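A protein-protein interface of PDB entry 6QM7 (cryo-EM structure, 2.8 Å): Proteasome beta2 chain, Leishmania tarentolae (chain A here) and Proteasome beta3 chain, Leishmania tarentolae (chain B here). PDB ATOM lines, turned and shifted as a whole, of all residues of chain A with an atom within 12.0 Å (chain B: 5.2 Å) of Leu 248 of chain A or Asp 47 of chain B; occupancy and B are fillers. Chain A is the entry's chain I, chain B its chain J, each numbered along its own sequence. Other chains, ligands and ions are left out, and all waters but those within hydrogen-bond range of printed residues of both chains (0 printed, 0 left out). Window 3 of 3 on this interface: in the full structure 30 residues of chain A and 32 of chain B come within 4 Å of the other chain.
Among the printed residues, merely in contact across the chains: Arg 246 of chain A with Lys 194 of chain B, Leu 248 of chain A with Lys 192 of chain B, Ile 245 of chain A with Lys 194 of chain B, Glu 244 of chain A with Val 195 of chain B, Gln 247 of chain A with Lys 194 of chain B, Ile 245 of chain A with Val 195 of chain B and Leu 248 of chain A with Asp 47 of chain B.
Printed residues of chain B within 4 Å of Leu 248 of chain A: Asp 47, Lys 192 and Asp 193. Asp 47 of chain B touches two residues of chain A. No residue of chain A comes within 4 Å of Asn 46 of chain B. No residue of chain A comes within 4 Å of Ser 48 of chain B. No residue of chain A comes within 4 Å of Ile 49 of chain B. No residue of chain A comes within 4 Å of Val 190 of chain B. Asp 193 of chain B touches two residues of chain A. Val 195 of chain B touches just these residues of chain A: Glu 244, Ile 245 and Arg 246. Of the printed residues of chain B, Arg 246 of chain A touches Asp 47 (3.3 Å), Lys 194 (3.3 Å) and Val 195 (2.9 Å). Of the printed residues of chain B, Ile 245 of chain A touches Lys 194 (3.7 Å) and Val 195 (3.9 Å). Of the printed residues of chain A, Lys 194 of chain B touches Ile 245 (3.7 Å), Arg 246 (3.3 Å) and Gln 247 (3.7 Å).
Of the 5 printed residues of chain A, 5 touch a printed residue of chain B. Among the printed residues, Asp or Glu carboxylates within 4 Å of a Lys or Arg side-chain nitrogen of the other chain: Arg 246 of chain A with Asp 47 of chain B (3.3 Å).
The side-chain carboxylate (OD1) of Asp 47 of chain B is in salt-bridge range of the guanidinium group (NH2) of Arg 246 of chain A (3.3 Å). NE2 of Gln 247 of chain A sits at hydrogen-bond distance from OD2 of Asp 193 of chain B, 3.0 Å away. N of Leu 248 of chain A lies within hydrogen-bond range of O of Asp 193 of chain B (2.9 Å). N of Val 195 of chain B is in hydrogen-bond range of O of Arg 246 of chain A (2.9 Å).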
ATOM      1  N   GLU A 244      -1.037  20.931  23.544  1.00  0.00           N
ATOM      2  CA  GLU A 244       0.339  20.376  23.635  1.00  0.00           C
ATOM      3  C   GLU A 244       1.292  21.515  23.995  1.00  0.00           C
ATOM      4  O   GLU A 244       1.485  22.411  23.148  1.00  0.00           O
ATOM      5  CB  GLU A 244       0.779  19.751  22.313  1.00  0.00           C
ATOM      6  CG  GLU A 244       0.033  18.477  21.964  1.00  0.00           C
ATOM      7  CD  GLU A 244       0.384  17.864  20.613  1.00  0.00           C
ATOM      8  OE1 GLU A 244       1.047  18.545  19.792  1.00  0.00           O
ATOM      9  OE2 GLU A 244      -0.013  16.698  20.383  1.00  0.00           O
ATOM     10  N   ILE A 245       1.845  21.491  25.207  1.00  0.00           N
ATOM     11  CA  ILE A 245       2.920  22.425  25.641  1.00  0.00           C
ATOM     12  C   ILE A 245       4.253  21.736  25.352  1.00  0.00           C
ATOM     13  O   ILE A 245       4.345  20.523  25.597  1.00  0.00           O
ATOM     14  CB  ILE A 245       2.769  22.827  27.120  1.00  0.00           C
ATOM     15  CG1 ILE A 245       1.400  23.465  27.395  1.00  0.00           C
ATOM     16  CG2 ILE A 245       3.916  23.742  27.539  1.00  0.00           C
ATOM     17  CD1 ILE A 245       1.075  23.673  28.865  1.00  0.00           C
ATOM     18  N   ARG A 246       5.215  22.483  24.809  1.00  0.00           N
ATOM     19  CA  ARG A 246       6.612  22.033  24.590  1.00  0.00           C
ATOM     20  C   ARG A 246       7.552  23.096  25.172  1.00  0.00           C
ATOM     21  O   ARG A 246       7.464  24.250  24.726  1.00  0.00           O
ATOM     22  CB  ARG A 246       6.863  21.800  23.098  1.00  0.00           C
ATOM     23  CG  ARG A 246       8.156  21.050  22.805  1.00  0.00           C
ATOM     24  CD  ARG A 246       8.415  20.847  21.323  1.00  0.00           C
ATOM     25  NE  ARG A 246       9.184  21.937  20.722  1.00  0.00           N
ATOM     26  CZ  ARG A 246       8.787  22.752  19.735  1.00  0.00           C
ATOM     27  NH1 ARG A 246       7.589  22.650  19.174  1.00  0.00           N
ATOM     28  NH2 ARG A 246       9.620  23.686  19.302  1.00  0.00           N
ATOM     29  N   GLN A 247       8.390  22.717  26.145  1.00  0.00           N
ATOM     30  CA  GLN A 247       9.414  23.593  26.783  1.00  0.00           C
ATOM     31  C   GLN A 247      10.699  23.549  25.946  1.00  0.00           C
ATOM     32  O   GLN A 247      10.921  22.526  25.264  1.00  0.00           O
ATOM     33  CB  GLN A 247       9.689  23.147  28.222  1.00  0.00           C
ATOM     34  CG  GLN A 247       8.469  23.193  29.140  1.00  0.00           C
ATOM     35  CD  GLN A 247       8.012  24.576  29.549  1.00  0.00           C
ATOM     36  OE1 GLN A 247       6.870  24.769  29.961  1.00  0.00           O
ATOM     37  NE2 GLN A 247       8.901  25.554  29.453  1.00  0.00           N
ATOM     38  N   LEU A 248      11.512  24.612  26.012  1.00  0.00           N
ATOM     39  CA  LEU A 248      12.785  24.777  25.250  1.00  0.00           C
ATOM     40  C   LEU A 248      13.930  25.075  26.233  1.00  0.00           C
ATOM     41  O   LEU A 248      14.733  24.210  26.601  1.00  0.00           O
ATOM     42  CB  LEU A 248      12.620  25.911  24.226  1.00  0.00           C
ATOM     43  CG  LEU A 248      11.318  25.921  23.417  1.00  0.00           C
ATOM     44  CD1 LEU A 248      11.154  27.229  22.652  1.00  0.00           C
ATOM     45  CD2 LEU A 248      11.260  24.740  22.460  1.00  0.00           C
ATOM     46  N   VAL B  44       5.880  24.498  11.143  1.00  0.00           N
ATOM     47  CA  VAL B  44       6.913  24.909  12.131  1.00  0.00           C
ATOM     48  C   VAL B  44       8.285  24.756  11.482  1.00  0.00           C
ATOM     49  O   VAL B  44       8.729  23.612  11.277  1.00  0.00           O
ATOM     50  CB  VAL B  44       6.791  24.102  13.427  1.00  0.00           C
ATOM     51  CG1 VAL B  44       7.943  24.388  14.374  1.00  0.00           C
ATOM     52  CG2 VAL B  44       5.460  24.389  14.089  1.00  0.00           C
ATOM     53  N   VAL B  45       8.917  25.886  11.185  1.00  0.00           N
ATOM     54  CA  VAL B  45      10.272  25.919  10.584  1.00  0.00           C
ATOM     55  C   VAL B  45      11.255  25.523  11.682  1.00  0.00           C
ATOM     56  O   VAL B  45      12.068  24.610  11.458  1.00  0.00           O
ATOM     57  CB  VAL B  45      10.599  27.300  10.002  1.00  0.00           C
ATOM     58  CG1 VAL B  45      11.971  27.297   9.347  1.00  0.00           C
ATOM     59  CG2 VAL B  45       9.539  27.788   9.026  1.00  0.00           C
ATOM     60  N   ASN B  46      11.157  26.179  12.832  1.00  0.00           N
ATOM     61  CA  ASN B  46      12.008  25.895  14.011  1.00  0.00           C
ATOM     62  C   ASN B  46      11.291  26.406  15.256  1.00  0.00           C
ATOM     63  O   ASN B  46      10.187  26.921  15.113  1.00  0.00           O
ATOM     64  CB  ASN B  46      13.409  26.485  13.825  1.00  0.00           C
ATOM     65  CG  ASN B  46      13.417  27.951  13.435  1.00  0.00           C
ATOM     66  OD1 ASN B  46      12.732  28.772  14.042  1.00  0.00           O
ATOM     67  ND2 ASN B  46      14.211  28.292  12.433  1.00  0.00           N
ATOM     68  N   ASP B  47      11.915  26.250  16.426  1.00  0.00           N
ATOM     69  CA  ASP B  47      11.449  26.759  17.747  1.00  0.00           C
ATOM     70  C   ASP B  47      10.777  28.126  17.592  1.00  0.00           C
ATOM     71  O   ASP B  47       9.668  28.313  18.118  1.00  0.00           O
ATOM     72  CB  ASP B  47      12.629  26.924  18.714  1.00  0.00           C
ATOM     73  CG  ASP B  47      13.259  25.633  19.226  1.00  0.00           C
ATOM     74  OD1 ASP B  47      12.795  24.536  18.821  1.00  0.00           O
ATOM     75  OD2 ASP B  47      14.210  25.737  20.047  1.00  0.00           O
ATOM     76  N   SER B  48      11.448  29.017  16.866  1.00  0.00           N
ATOM     77  CA  SER B  48      11.236  30.480  16.870  1.00  0.00           C
ATOM     78  C   SER B  48      10.329  30.939  15.716  1.00  0.00           C
ATOM     79  O   SER B  48       9.765  32.032  15.846  1.00  0.00           O
ATOM     80  CB  SER B  48      12.574  31.182  16.839  1.00  0.00           C
ATOM     81  OG  SER B  48      12.788  31.835  15.590  1.00  0.00           O
ATOM     82  N   ILE B  49      10.212  30.178  14.624  1.00  0.00           N
ATOM     83  CA  ILE B  49       9.396  30.564  13.436  1.00  0.00           C
ATOM     84  C   ILE B  49       8.264  29.562  13.218  1.00  0.00           C
ATOM     85  O   ILE B  49       8.537  28.363  13.127  1.00  0.00           O
ATOM     86  CB  ILE B  49      10.239  30.630  12.157  1.00  0.00           C
ATOM     87  CG1 ILE B  49      11.468  31.520  12.292  1.00  0.00           C
ATOM     88  CG2 ILE B  49       9.380  31.055  10.971  1.00  0.00           C
ATOM     89  CD1 ILE B  49      12.455  31.287  11.177  1.00  0.00           C
ATOM     90  N   LYS B 114      15.110  34.645  19.833  1.00  0.00           N
ATOM     91  CA  LYS B 114      15.199  33.828  21.073  1.00  0.00           C
ATOM     92  C   LYS B 114      15.860  34.645  22.195  1.00  0.00           C
ATOM     93  O   LYS B 114      15.457  34.460  23.363  1.00  0.00           O
ATOM     94  CB  LYS B 114      15.956  32.527  20.787  1.00  0.00           C
ATOM     95  CG  LYS B 114      15.650  31.396  21.759  1.00  0.00           C
ATOM     96  CD  LYS B 114      16.528  30.177  21.576  1.00  0.00           C
ATOM     97  CE  LYS B 114      16.036  28.986  22.371  1.00  0.00           C
ATOM     98  NZ  LYS B 114      17.127  28.019  22.635  1.00  0.00           N
ATOM     99  N   VAL B 190       3.809  30.973  20.613  1.00  0.00           N
ATOM    100  CA  VAL B 190       5.287  30.871  20.638  1.00  0.00           C
ATOM    101  C   VAL B 190       5.806  31.952  21.584  1.00  0.00           C
ATOM    102  O   VAL B 190       5.351  33.094  21.484  1.00  0.00           O
ATOM    103  CB  VAL B 190       5.877  30.964  19.222  1.00  0.00           C
ATOM    104  CG1 VAL B 190       7.391  30.807  19.232  1.00  0.00           C
ATOM    105  CG2 VAL B 190       5.256  29.921  18.304  1.00  0.00           C
ATOM    106  N   THR B 191       6.669  31.547  22.516  1.00  0.00           N
ATOM    107  CA  THR B 191       7.360  32.391  23.524  1.00  0.00           C
ATOM    108  C   THR B 191       8.855  32.092  23.379  1.00  0.00           C
ATOM    109  O   THR B 191       9.193  31.234  22.536  1.00  0.00           O
ATOM    110  CB  THR B 191       6.750  32.117  24.907  1.00  0.00           C
ATOM    111  OG1 THR B 191       5.329  32.209  24.790  1.00  0.00           O
ATOM    112  CG2 THR B 191       7.201  33.078  25.983  1.00  0.00           C
ATOM    113  N   LYS B 192       9.731  32.783  24.104  1.00  0.00           N
ATOM    114  CA  LYS B 192      11.178  32.426  24.149  1.00  0.00           C
ATOM    115  C   LYS B 192      11.297  31.045  24.811  1.00  0.00           C
ATOM    116  O   LYS B 192      12.034  30.186  24.293  1.00  0.00           O
ATOM    117  CB  LYS B 192      12.010  33.463  24.916  1.00  0.00           C
ATOM    118  CG  LYS B 192      11.596  34.923  24.754  1.00  0.00           C
ATOM    119  CD  LYS B 192      12.739  35.924  24.899  1.00  0.00           C
ATOM    120  CE  LYS B 192      13.431  35.904  26.247  1.00  0.00           C
ATOM    121  NZ  LYS B 192      12.539  36.391  27.328  1.00  0.00           N
ATOM    122  N   ASP B 193      10.561  30.858  25.908  1.00  0.00           N
ATOM    123  CA  ASP B 193      10.671  29.714  26.845  1.00  0.00           C
ATOM    124  C   ASP B 193       9.986  28.485  26.236  1.00  0.00           C
ATOM    125  O   ASP B 193      10.618  27.413  26.241  1.00  0.00           O
ATOM    126  CB  ASP B 193      10.082  30.093  28.213  1.00  0.00           C
ATOM    127  CG  ASP B 193      10.154  28.999  29.276  1.00  0.00           C
ATOM    128  OD1 ASP B 193      11.285  28.583  29.614  1.00  0.00           O
ATOM    129  OD2 ASP B 193       9.079  28.568  29.761  1.00  0.00           O
ATOM    130  N   LYS B 194       8.739  28.613  25.768  1.00  0.00           N
ATOM    131  CA  LYS B 194       7.901  27.448  25.374  1.00  0.00           C
ATOM    132  C   LYS B 194       6.974  27.757  24.198  1.00  0.00           C
ATOM    133  O   LYS B 194       6.639  28.928  23.974  1.00  0.00           O
ATOM    134  CB  LYS B 194       7.047  26.960  26.545  1.00  0.00           C
ATOM    135  CG  LYS B 194       6.091  27.972  27.159  1.00  0.00           C
ATOM    136  CD  LYS B 194       4.856  27.314  27.754  1.00  0.00           C
ATOM    137  CE  LYS B 194       3.925  28.289  28.445  1.00  0.00           C
ATOM    138  NZ  LYS B 194       4.328  28.519  29.852  1.00  0.00           N
ATOM    139  N   VAL B 195       6.540  26.690  23.529  1.00  0.00           N
ATOM    140  CA  VAL B 195       5.579  26.689  22.391  1.00  0.00           C
ATOM    141  C   VAL B 195       4.350  25.874  22.793  1.00  0.00           C
ATOM    142  O   VAL B 195       4.421  24.640  22.805  1.00  0.00           O
ATOM    143  CB  VAL B 195       6.229  26.109  21.126  1.00  0.00           C
ATOM    144  CG1 VAL B 195       5.232  26.014  19.981  1.00  0.00           C
ATOM    145  CG2 VAL B 195       7.460  26.906  20.723  1.00  0.00           C
